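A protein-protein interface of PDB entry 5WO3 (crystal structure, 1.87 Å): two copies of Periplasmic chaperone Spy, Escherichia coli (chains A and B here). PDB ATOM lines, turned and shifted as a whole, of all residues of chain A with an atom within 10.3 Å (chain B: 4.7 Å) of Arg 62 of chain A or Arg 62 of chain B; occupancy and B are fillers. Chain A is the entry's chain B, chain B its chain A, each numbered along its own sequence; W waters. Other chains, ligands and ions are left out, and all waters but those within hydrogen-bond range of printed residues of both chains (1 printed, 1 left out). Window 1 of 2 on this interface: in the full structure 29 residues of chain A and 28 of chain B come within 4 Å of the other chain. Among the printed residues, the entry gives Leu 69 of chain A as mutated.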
ATOM      1  N   GLU A  33       4.251 -26.396 -20.257  1.00  0.00           N
ATOM      2  CA  GLU A  33       4.365 -26.170 -21.697  1.00  0.00           C
ATOM      3  C   GLU A  33       3.472 -27.121 -22.469  1.00  0.00           C
ATOM      4  O   GLU A  33       2.687 -26.704 -23.338  1.00  0.00           O
ATOM      5  CB  GLU A  33       5.823 -26.344 -22.133  1.00  0.00           C
ATOM      6  CG  GLU A  33       6.065 -26.436 -23.639  1.00  0.00           C
ATOM      7  CD  GLU A  33       7.139 -27.460 -23.980  1.00  0.00           C
ATOM      8  OE1 GLU A  33       6.786 -28.668 -24.089  1.00  0.00           O
ATOM      9  OE2 GLU A  33       8.323 -27.054 -24.131  1.00  0.00           O
ATOM     10  N   MET A  37       0.149 -26.825 -24.885  1.00  0.00           N
ATOM     11  CA  MET A  37      -0.002 -27.504 -26.176  1.00  0.00           C
ATOM     12  C   MET A  37      -1.289 -28.290 -26.233  1.00  0.00           C
ATOM     13  O   MET A  37      -2.018 -28.303 -27.239  1.00  0.00           O
ATOM     14  CB  MET A  37       1.189 -28.440 -26.412  1.00  0.00           C
ATOM     15  CG  MET A  37       1.132 -29.268 -27.695  1.00  0.00           C
ATOM     16  SD  MET A  37       1.445 -28.269 -29.154  1.00  0.00           S
ATOM     17  CE  MET A  37       3.218 -28.365 -29.265  1.00  0.00           C
ATOM     18  N   ALA A  51      -1.305 -19.952 -30.728  1.00  0.00           N
ATOM     19  CA  ALA A  51      -0.285 -20.953 -31.067  1.00  0.00           C
ATOM     20  C   ALA A  51       1.087 -20.273 -31.209  1.00  0.00           C
ATOM     21  O   ALA A  51       2.089 -20.801 -30.750  1.00  0.00           O
ATOM     22  CB  ALA A  51      -0.646 -21.655 -32.325  1.00  0.00           C
ATOM     23  N   GLU A  52       1.122 -19.124 -31.867  1.00  0.00           N
ATOM     24  CA  GLU A  52       2.385 -18.428 -32.047  1.00  0.00           C
ATOM     25  C   GLU A  52       2.957 -18.064 -30.680  1.00  0.00           C
ATOM     26  O   GLU A  52       4.185 -18.129 -30.489  1.00  0.00           O
ATOM     27  CB  GLU A  52       2.244 -17.179 -32.915  1.00  0.00           C
ATOM     28  CG  GLU A  52       1.938 -17.470 -34.383  1.00  0.00           C
ATOM     29  CD  GLU A  52       1.671 -16.217 -35.169  1.00  0.00           C
ATOM     30  OE1 GLU A  52       0.876 -15.342 -34.772  1.00  0.00           O
ATOM     31  OE2 GLU A  52       2.285 -16.105 -36.191  1.00  0.00           O
ATOM     32  N   GLN A  54       2.635 -19.693 -27.871  1.00  0.00           N
ATOM     33  CA  GLN A  54       3.113 -20.938 -27.271  1.00  0.00           C
ATOM     34  C   GLN A  54       4.451 -21.321 -27.921  1.00  0.00           C
ATOM     35  O   GLN A  54       5.389 -21.660 -27.219  1.00  0.00           O
ATOM     36  CB  GLN A  54       2.084 -22.075 -27.440  1.00  0.00           C
ATOM     37  CG  GLN A  54       2.401 -23.332 -26.663  1.00  0.00           C
ATOM     38  CD  GLN A  54       2.742 -23.044 -25.206  1.00  0.00           C
ATOM     39  OE1 GLN A  54       2.167 -22.146 -24.578  1.00  0.00           O
ATOM     40  NE2 GLN A  54       3.699 -23.797 -24.667  1.00  0.00           N
ATOM     41  N   ILE A  55       4.543 -21.261 -29.249  1.00  0.00           N
ATOM     42  CA  ILE A  55       5.809 -21.524 -29.944  1.00  0.00           C
ATOM     43  C   ILE A  55       6.940 -20.622 -29.417  1.00  0.00           C
ATOM     44  O   ILE A  55       8.057 -21.070 -29.099  1.00  0.00           O
ATOM     45  CB  ILE A  55       5.648 -21.345 -31.491  1.00  0.00           C
ATOM     46  CG1 ILE A  55       4.794 -22.477 -32.073  1.00  0.00           C
ATOM     47  CG2 ILE A  55       6.974 -21.313 -32.197  1.00  0.00           C
ATOM     48  CD1 ILE A  55       4.220 -22.208 -33.451  1.00  0.00           C
ATOM     49  N   ALA A  56       6.660 -19.338 -29.311  1.00  0.00           N
ATOM     50  CA  ALA A  56       7.673 -18.424 -28.815  1.00  0.00           C
ATOM     51  C   ALA A  56       8.109 -18.745 -27.387  1.00  0.00           C
ATOM     52  O   ALA A  56       9.316 -18.727 -27.071  1.00  0.00           O
ATOM     53  CB  ALA A  56       7.186 -16.986 -28.900  1.00  0.00           C
ATOM     54  N   LYS A  57       7.158 -19.064 -26.522  1.00  0.00           N
ATOM     55  CA  LYS A  57       7.493 -19.468 -25.159  1.00  0.00           C
ATOM     56  C   LYS A  57       8.381 -20.703 -25.161  1.00  0.00           C
ATOM     57  O   LYS A  57       9.377 -20.786 -24.427  1.00  0.00           O
ATOM     58  CB  LYS A  57       6.227 -19.707 -24.330  1.00  0.00           C
ATOM     59  CG  LYS A  57       6.481 -19.922 -22.856  1.00  0.00           C
ATOM     60  CD  LYS A  57       5.152 -19.994 -22.089  1.00  0.00           C
ATOM     61  CE  LYS A  57       5.379 -20.297 -20.603  1.00  0.00           C
ATOM     62  NZ  LYS A  57       4.099 -20.254 -19.810  1.00  0.00           N
ATOM     63  N   MET A  58       8.074 -21.638 -26.040  1.00  0.00           N
ATOM     64  CA  MET A  58       8.866 -22.856 -26.137  1.00  0.00           C
ATOM     65  C   MET A  58      10.311 -22.631 -26.563  1.00  0.00           C
ATOM     66  O   MET A  58      11.191 -23.443 -26.236  1.00  0.00           O
ATOM     67  CB  MET A  58       8.209 -23.800 -27.132  1.00  0.00           C
ATOM     68  CG  MET A  58       7.006 -24.539 -26.588  1.00  0.00           C
ATOM     69  SD  MET A  58       6.068 -25.275 -27.950  1.00  0.00           S
ATOM     70  CE  MET A  58       6.864 -26.881 -28.093  1.00  0.00           C
ATOM     71  N   GLU A  59      10.559 -21.553 -27.305  1.00  0.00           N
ATOM     72  CA  GLU A  59      11.925 -21.195 -27.736  1.00  0.00           C
ATOM     73  C   GLU A  59      12.852 -20.937 -26.560  1.00  0.00           C
ATOM     74  O   GLU A  59      14.055 -21.147 -26.670  1.00  0.00           O
ATOM     75  CB  GLU A  59      11.932 -19.965 -28.632  1.00  0.00           C
ATOM     76  CG  GLU A  59      11.371 -20.213 -30.021  1.00  0.00           C
ATOM     77  CD  GLU A  59      12.297 -20.980 -30.983  1.00  0.00           C
ATOM     78  OE1 GLU A  59      13.543 -20.830 -30.949  1.00  0.00           O
ATOM     79  OE2 GLU A  59      11.764 -21.703 -31.845  1.00  0.00           O
ATOM     80  N   GLU A  60      12.301 -20.491 -25.444  1.00  0.00           N
ATOM     81  CA  GLU A  60      13.119 -20.155 -24.281  1.00  0.00           C
ATOM     82  C   GLU A  60      13.664 -21.444 -23.675  1.00  0.00           C
ATOM     83  O   GLU A  60      14.838 -21.514 -23.361  1.00  0.00           O
ATOM     84  CB  GLU A  60      12.288 -19.321 -23.277  1.00  0.00           C
ATOM     85  CG  GLU A  60      12.941 -18.963 -21.932  1.00  0.00           C
ATOM     86  CD  GLU A  60      14.226 -18.095 -22.008  1.00  0.00           C
ATOM     87  OE1 GLU A  60      14.619 -17.601 -23.084  1.00  0.00           O
ATOM     88  OE2 GLU A  60      14.864 -17.921 -20.944  1.00  0.00           O
ATOM     89  N   GLN A  61      12.835 -22.478 -23.559  1.00  0.00           N
ATOM     90  CA  GLN A  61      13.273 -23.725 -22.934  1.00  0.00           C
ATOM     91  C   GLN A  61      14.183 -24.499 -23.889  1.00  0.00           C
ATOM     92  O   GLN A  61      15.106 -25.199 -23.458  1.00  0.00           O
ATOM     93  CB  GLN A  61      12.050 -24.578 -22.505  1.00  0.00           C
ATOM     94  CG  GLN A  61      12.375 -25.784 -21.655  1.00  0.00           C
ATOM     95  CD  GLN A  61      13.137 -25.414 -20.400  1.00  0.00           C
ATOM     96  OE1 GLN A  61      12.777 -24.470 -19.694  1.00  0.00           O
ATOM     97  NE2 GLN A  61      14.215 -26.140 -20.131  1.00  0.00           N
ATOM     98  N   ARG A  62      13.929 -24.357 -25.185  1.00  0.00           N
ATOM     99  CA  ARG A  62      14.746 -25.018 -26.182  1.00  0.00           C
ATOM    100  C   ARG A  62      16.172 -24.441 -26.161  1.00  0.00           C
ATOM    101  O   ARG A  62      17.139 -25.165 -26.238  1.00  0.00           O
ATOM    102  CB  ARG A  62      14.138 -24.890 -27.581  1.00  0.00           C
ATOM    103  CG  ARG A  62      15.100 -25.255 -28.695  1.00  0.00           C
ATOM    104  CD  ARG A  62      14.428 -25.400 -30.050  1.00  0.00           C
ATOM    105  NE  ARG A  62      15.362 -25.897 -31.060  1.00  0.00           N
ATOM    106  CZ  ARG A  62      16.302 -25.139 -31.625  1.00  0.00           C
ATOM    107  NH1 ARG A  62      16.417 -23.864 -31.261  1.00  0.00           N
ATOM    108  NH2 ARG A  62      17.130 -25.632 -32.542  1.00  0.00           N
ATOM    109  N   LYS A  63      16.268 -23.121 -26.059  1.00  0.00           N
ATOM    110  CA  LYS A  63      17.529 -22.461 -25.921  1.00  0.00           C
ATOM    111  C   LYS A  63      18.279 -23.023 -24.726  1.00  0.00           C
ATOM    112  O   LYS A  63      19.461 -23.429 -24.822  1.00  0.00           O
ATOM    113  CB  LYS A  63      17.310 -20.961 -25.783  1.00  0.00           C
ATOM    114  CG  LYS A  63      18.603 -20.144 -25.674  1.00  0.00           C
ATOM    115  CD  LYS A  63      18.357 -18.651 -25.429  1.00  0.00           C
ATOM    116  CE  LYS A  63      18.553 -18.282 -23.990  1.00  0.00           C
ATOM    117  NZ  LYS A  63      18.117 -16.867 -23.701  1.00  0.00           N
ATOM    118  N   ALA A  64      17.610 -23.072 -23.589  1.00  0.00           N
ATOM    119  CA  ALA A  64      18.290 -23.518 -22.371  1.00  0.00           C
ATOM    120  C   ALA A  64      18.788 -24.955 -22.552  1.00  0.00           C
ATOM    121  O   ALA A  64      19.932 -25.281 -22.205  1.00  0.00           O
ATOM    122  CB  ALA A  64      17.381 -23.419 -21.212  1.00  0.00           C
ATOM    123  N   ASN A  65      17.922 -25.802 -23.115  1.00  0.00           N
ATOM    124  CA  ASN A  65      18.258 -27.201 -23.371  1.00  0.00           C
ATOM    125  C   ASN A  65      19.356 -27.433 -24.383  1.00  0.00           C
ATOM    126  O   ASN A  65      20.232 -28.252 -24.153  1.00  0.00           O
ATOM    127  CB  ASN A  65      17.012 -27.970 -23.820  1.00  0.00           C
ATOM    128  CG  ASN A  65      15.969 -28.074 -22.720  1.00  0.00           C
ATOM    129  OD1 ASN A  65      16.297 -28.004 -21.533  1.00  0.00           O
ATOM    130  ND2 ASN A  65      14.707 -28.247 -23.108  1.00  0.00           N
ATOM    131  N   MET A  66      19.324 -26.714 -25.493  1.00  0.00           N
ATOM    132  CA  MET A  66      20.334 -26.885 -26.516  1.00  0.00           C
ATOM    133  C   MET A  66      21.677 -26.358 -26.039  1.00  0.00           C
ATOM    134  O   MET A  66      22.717 -26.861 -26.440  1.00  0.00           O
ATOM    135  CB  MET A  66      19.922 -26.173 -27.805  1.00  0.00           C
ATOM    136  CG  MET A  66      18.740 -26.837 -28.547  1.00  0.00           C
ATOM    137  SD  MET A  66      19.061 -28.591 -28.822  1.00  0.00           S
ATOM    138  CE  MET A  66      20.759 -28.547 -29.356  1.00  0.00           C
ATOM    139  N   LEU A  67      21.662 -25.328 -25.199  1.00  0.00           N
ATOM    140  CA  LEU A  67      22.918 -24.797 -24.642  1.00  0.00           C
ATOM    141  C   LEU A  67      23.562 -25.803 -23.681  1.00  0.00           C
ATOM    142  O   LEU A  67      24.737 -25.992 -23.712  1.00  0.00           O
ATOM    143  CB  LEU A  67      22.706 -23.488 -23.905  1.00  0.00           C
ATOM    144  CG  LEU A  67      22.619 -22.222 -24.736  1.00  0.00           C
ATOM    145  CD1 LEU A  67      22.155 -20.990 -23.888  1.00  0.00           C
ATOM    146  CD2 LEU A  67      23.944 -21.928 -25.398  1.00  0.00           C
ATOM    147  N   ALA A  68      22.766 -26.453 -22.846  1.00  0.00           N
ATOM    148  CA  ALA A  68      23.295 -27.422 -21.885  1.00  0.00           C
ATOM    149  C   ALA A  68      23.827 -28.628 -22.627  1.00  0.00           C
ATOM    150  O   ALA A  68      24.854 -29.170 -22.307  1.00  0.00           O
ATOM    151  CB  ALA A  68      22.220 -27.844 -20.912  1.00  0.00           C
ATOM    152  N   LEU A  69      23.093 -29.059 -23.651  1.00  0.00           N
ATOM    153  CA  LEU A  69      23.486 -30.215 -24.460  1.00  0.00           C
ATOM    154  C   LEU A  69      24.801 -29.953 -25.188  1.00  0.00           C
ATOM    155  O   LEU A  69      25.733 -30.767 -25.131  1.00  0.00           O
ATOM    156  CB  LEU A  69      22.359 -30.532 -25.458  1.00  0.00           C
ATOM    157  CG  LEU A  69      22.395 -31.346 -26.782  1.00  0.00           C
ATOM    158  CD1 LEU A  69      23.745 -31.500 -27.485  1.00  0.00           C
ATOM    159  CD2 LEU A  69      21.718 -32.707 -26.644  1.00  0.00           C
ATOM    160  N   MET A  70      24.888 -28.835 -25.904  1.00  0.00           N
ATOM    161  CA  MET A  70      26.139 -28.504 -26.570  1.00  0.00           C
ATOM    162  C   MET A  70      27.303 -28.314 -25.601  1.00  0.00           C
ATOM    163  O   MET A  70      28.395 -28.764 -25.882  1.00  0.00           O
ATOM    164  CB  MET A  70      25.971 -27.243 -27.441  1.00  0.00           C
ATOM    165  CG  MET A  70      25.199 -27.502 -28.744  1.00  0.00           C
ATOM    166  SD  MET A  70      25.137 -26.119 -29.922  1.00  0.00           S
ATOM    167  CE  MET A  70      23.693 -25.382 -29.278  1.00  0.00           C
ATOM    168  N   GLU B  33      22.222 -27.265 -40.163  1.00  0.00           N
ATOM    169  CA  GLU B  33      22.123 -26.966 -38.746  1.00  0.00           C
ATOM    170  C   GLU B  33      22.983 -27.940 -37.929  1.00  0.00           C
ATOM    171  O   GLU B  33      23.634 -27.532 -36.978  1.00  0.00           O
ATOM    172  CB  GLU B  33      20.658 -26.998 -38.260  1.00  0.00           C
ATOM    173  CG  GLU B  33      20.533 -26.349 -36.861  1.00  0.00           C
ATOM    174  CD  GLU B  33      19.116 -26.267 -36.286  1.00  0.00           C
ATOM    175  OE1 GLU B  33      18.255 -27.111 -36.631  1.00  0.00           O
ATOM    176  OE2 GLU B  33      18.875 -25.346 -35.467  1.00  0.00           O
ATOM    177  N   ILE B  55      21.529 -21.592 -32.272  1.00  0.00           N
ATOM    178  CA  ILE B  55      20.269 -22.096 -31.721  1.00  0.00           C
ATOM    179  C   ILE B  55      19.132 -21.249 -32.283  1.00  0.00           C
ATOM    180  O   ILE B  55      18.070 -21.749 -32.607  1.00  0.00           O
ATOM    181  CB  ILE B  55      20.302 -22.054 -30.179  1.00  0.00           C
ATOM    182  CG1 ILE B  55      21.230 -23.132 -29.650  1.00  0.00           C
ATOM    183  CG2 ILE B  55      18.925 -22.189 -29.565  1.00  0.00           C
ATOM    184  CD1 ILE B  55      21.510 -22.955 -28.182  1.00  0.00           C
ATOM    185  N   ALA B  56      19.402 -19.961 -32.459  1.00  0.00           N
ATOM    186  CA  ALA B  56      18.381 -19.014 -32.922  1.00  0.00           C
ATOM    187  C   ALA B  56      18.139 -19.010 -34.414  1.00  0.00           C
ATOM    188  O   ALA B  56      17.101 -18.514 -34.874  1.00  0.00           O
ATOM    189  CB  ALA B  56      18.747 -17.620 -32.503  1.00  0.00           C
ATOM    190  N   MET B  58      17.308 -21.017 -36.965  1.00  0.00           N
ATOM    191  CA  MET B  58      16.138 -21.550 -37.673  1.00  0.00           C
ATOM    192  C   MET B  58      14.809 -21.260 -36.933  1.00  0.00           C
ATOM    193  O   MET B  58      13.827 -21.976 -37.095  1.00  0.00           O
ATOM    194  CB  MET B  58      16.312 -23.050 -37.898  1.00  0.00           C
ATOM    195  CG  MET B  58      17.587 -23.431 -38.685  1.00  0.00           C
ATOM    196  SD  MET B  58      17.876 -22.510 -40.223  1.00  0.00           S
ATOM    197  CE  MET B  58      16.432 -22.962 -41.187  1.00  0.00           C
ATOM    198  N   GLU B  59      14.772 -20.171 -36.168  1.00  0.00           N
ATOM    199  CA  GLU B  59      13.557 -19.808 -35.456  1.00  0.00           C
ATOM    200  C   GLU B  59      12.324 -19.734 -36.399  1.00  0.00           C
ATOM    201  O   GLU B  59      11.258 -20.298 -36.110  1.00  0.00           O
ATOM    202  CB  GLU B  59      13.779 -18.485 -34.753  1.00  0.00           C
ATOM    203  CG  GLU B  59      12.617 -17.950 -34.007  1.00  0.00           C
ATOM    204  CD  GLU B  59      12.921 -16.538 -33.480  1.00  0.00           C
ATOM    205  OE1 GLU B  59      14.006 -16.392 -32.868  1.00  0.00           O
ATOM    206  OE2 GLU B  59      12.080 -15.616 -33.675  1.00  0.00           O
ATOM    207  N   GLU B  60      12.470 -19.068 -37.539  1.00  0.00           N
ATOM    208  CA  GLU B  60      11.321 -18.878 -38.467  1.00  0.00           C
ATOM    209  C   GLU B  60      10.838 -20.196 -39.048  1.00  0.00           C
ATOM    210  O   GLU B  60       9.646 -20.454 -39.116  1.00  0.00           O
ATOM    211  CB  GLU B  60      11.694 -17.929 -39.602  1.00  0.00           C
ATOM    212  N   GLN B  61      11.764 -21.042 -39.469  1.00  0.00           N
ATOM    213  CA  GLN B  61      11.395 -22.358 -39.980  1.00  0.00           C
ATOM    214  C   GLN B  61      10.749 -23.226 -38.887  1.00  0.00           C
ATOM    215  O   GLN B  61       9.776 -23.965 -39.145  1.00  0.00           O
ATOM    216  CB  GLN B  61      12.648 -23.047 -40.578  1.00  0.00           C
ATOM    217  N   ARG B  62      11.281 -23.156 -37.668  1.00  0.00           N
ATOM    218  CA  ARG B  62      10.707 -23.904 -36.561  1.00  0.00           C
ATOM    219  C   ARG B  62       9.254 -23.480 -36.301  1.00  0.00           C
ATOM    220  O   ARG B  62       8.379 -24.320 -36.052  1.00  0.00           O
ATOM    221  CB  ARG B  62      11.523 -23.705 -35.301  1.00  0.00           C
ATOM    222  CG  ARG B  62      12.755 -24.578 -35.217  1.00  0.00           C
ATOM    223  CD  ARG B  62      13.314 -24.574 -33.805  1.00  0.00           C
ATOM    224  NE  ARG B  62      13.731 -23.229 -33.356  1.00  0.00           N
ATOM    225  CZ  ARG B  62      14.933 -22.717 -33.593  1.00  0.00           C
ATOM    226  NH1 ARG B  62      15.831 -23.418 -34.289  1.00  0.00           N
ATOM    227  NH2 ARG B  62      15.248 -21.510 -33.133  1.00  0.00           N
ATOM    228  N   LYS B  63       9.029 -22.175 -36.351  1.00  0.00           N
ATOM    229  CA  LYS B  63       7.703 -21.589 -36.180  1.00  0.00           C
ATOM    230  C   LYS B  63       6.738 -22.105 -37.231  1.00  0.00           C
ATOM    231  O   LYS B  63       5.652 -22.593 -36.899  1.00  0.00           O
ATOM    232  CB  LYS B  63       7.788 -20.072 -36.257  1.00  0.00           C
ATOM    233  CG  LYS B  63       6.435 -19.336 -36.078  1.00  0.00           C
ATOM    234  CD  LYS B  63       6.597 -17.843 -36.135  1.00  0.00           C
ATOM    235  CE  LYS B  63       5.231 -17.161 -36.024  1.00  0.00           C
ATOM    236  NZ  LYS B  63       5.371 -15.672 -36.221  1.00  0.00           N
ATOM    237  N   ALA B  64       7.148 -22.037 -38.496  1.00  0.00           N
ATOM    238  CA  ALA B  64       6.251 -22.442 -39.586  1.00  0.00           C
ATOM    239  C   ALA B  64       5.911 -23.905 -39.424  1.00  0.00           C
ATOM    240  O   ALA B  64       4.761 -24.307 -39.598  1.00  0.00           O
ATOM    241  CB  ALA B  64       6.882 -22.164 -40.924  1.00  0.00           C
ATOM    242  N   ASN B  65       6.908 -24.725 -39.090  1.00  0.00           N
ATOM    243  CA  ASN B  65       6.664 -26.173 -39.016  1.00  0.00           C
ATOM    244  C   ASN B  65       5.777 -26.530 -37.858  1.00  0.00           C
ATOM    245  O   ASN B  65       4.888 -27.352 -37.978  1.00  0.00           O
ATOM    246  CB  ASN B  65       7.975 -26.947 -38.905  1.00  0.00           C
ATOM    247  CG  ASN B  65       8.771 -26.898 -40.182  1.00  0.00           C
ATOM    248  OD1 ASN B  65       8.216 -26.664 -41.258  1.00  0.00           O
ATOM    249  ND2 ASN B  65      10.073 -27.119 -40.083  1.00  0.00           N
ATOM    250  N   MET B  66       6.008 -25.883 -36.730  1.00  0.00           N
ATOM    251  CA  MET B  66       5.190 -26.137 -35.560  1.00  0.00           C
ATOM    252  C   MET B  66       3.794 -25.638 -35.711  1.00  0.00           C
ATOM    253  O   MET B  66       2.867 -26.284 -35.243  1.00  0.00           O
ATOM    254  CB  MET B  66       5.815 -25.481 -34.316  1.00  0.00           C
ATOM    255  CG  MET B  66       5.134 -25.862 -33.014  1.00  0.00           C
ATOM    256  SD  MET B  66       5.191 -27.633 -32.721  1.00  0.00           S
ATOM    257  CE  MET B  66       6.967 -27.924 -32.799  1.00  0.00           C
HETATM  258  O   HOH W   1      10.095 -20.585 -33.472  1.00  0.00           O
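The guanidinium group of Arg 62 of chain B lies close to the guanidinium group of Arg 62 of chain A (3.1 Å). The side-chain carboxylate (OE2) of Glu 33 of chain B lies within salt-bridge range of the guanidinium group (NH2) of Arg 62 of chain A. NH1 of Arg 62 of chain A is in hydrogen-bond range of O of Ile 55 of chain B (3.0 Å). The side-chain carboxylate (OE2) of Glu 52 of chain A is in salt-bridge range of the side-chain amino group (NZ) of Lys 63 of chain B (3.1 Å). The guanidinium group of Arg 62 of chain B is in salt-bridge range of the side-chain carboxylate of Glu 59 of chain A (2.9 Å).
Among the printed residues, merely in contact across the chains: Met 70 of chain A with Ile 55 of chain B, Ile 55 of chain A with Met 66 of chain B, Met 66 of chain A with Ile 55 of chain B, Leu 67 of chain A with Ile 55 of chain B, Ile 55 of chain A with Lys 63 of chain B and Lys 63 of chain A with Ile 55 of chain B.
Gln 54 of chain A touches none of the printed residues of chain B. Of chain B, only Glu 33, Ile 55 and Arg 62 come within 4 Å of Arg 62 of chain A. Of the printed residues of chain B, Leu 67 of chain A touches Ile 55. Leu 69 of chain A touches none of the printed residues of chain B. Printed residues of chain B within 4 Å of Met 70 of chain A: Ile 55 (3.4 Å). Of the printed residues of chain A, Glu 33 of chain B touches Arg 62 (3.4 Å). No residue of chain A comes within 4 Å of Glu 60 of chain B. Arg 62 of chain B touches just these residues of chain A: Glu 59 and Arg 62. No residue of chain A comes within 4 Å of Asn 65 of chain B. Of chain A, only Ile 55 comes within 4 Å of Met 66 of chain B. The nearest residue of chain A that does not touch Arg 62 of chain B is Ile 55 of chain A (5.1 Å).
Of the 21 printed residues of chain A, 8 touch a printed residue of chain B. Of the 12 printed residues of chain B, 5 touch a printed residue of chain A. Along chain B the printed residues that touch a printed residue of chain A span positions 33 to 66. Among the printed residues, 11 pairs touch across the chains. Among the printed residues, Asp or Glu carboxylates within 4 Å of a Lys or Arg side-chain nitrogen of the other chain: Glu 52 of chain A with Lys 63 of chain B (3.1 Å), Glu 59 of chain A with Arg 62 of chain B (2.9 Å) and Arg 62 of chain A with Glu 33 of chain B (3.4 Å).
Ile 55 of chain A touches Lys 63 of chain B, and with the chains exchanged Lys 63 of chain A touches Ile 55 of chain B. Ile 55 of chain A touches Met 66 of chain B, and with the chains exchanged Met 66 of chain A touches Ile 55 of chain B. Arg 62 of chain A touches Ile 55 of chain B, but with the chains exchanged Ile 55 of chain A does not touch Arg 62 of chain B (5.1 Å). Arg 62 of chain B touches its own counterpart, Arg 62 of chain A.
Water W1 lies within hydrogen-bond range of OE2 of Glu 59 of chain A (2.6 Å), O of Glu 59 of chain B (2.9 Å) and N of Lys 63 of chain B (3.5 Å).
NZ of Lys 63 of chain A sits close to OE1 of Glu 60 of chain A (3.6 Å). OE2 of Glu 33 of chain B lies within salt-bridge range of NH1 of Arg 62 of chain B. NH2 of Arg 62 of chain B lies within hydrogen-bond range of O of Ile 55 of chain B (2.9 Å).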
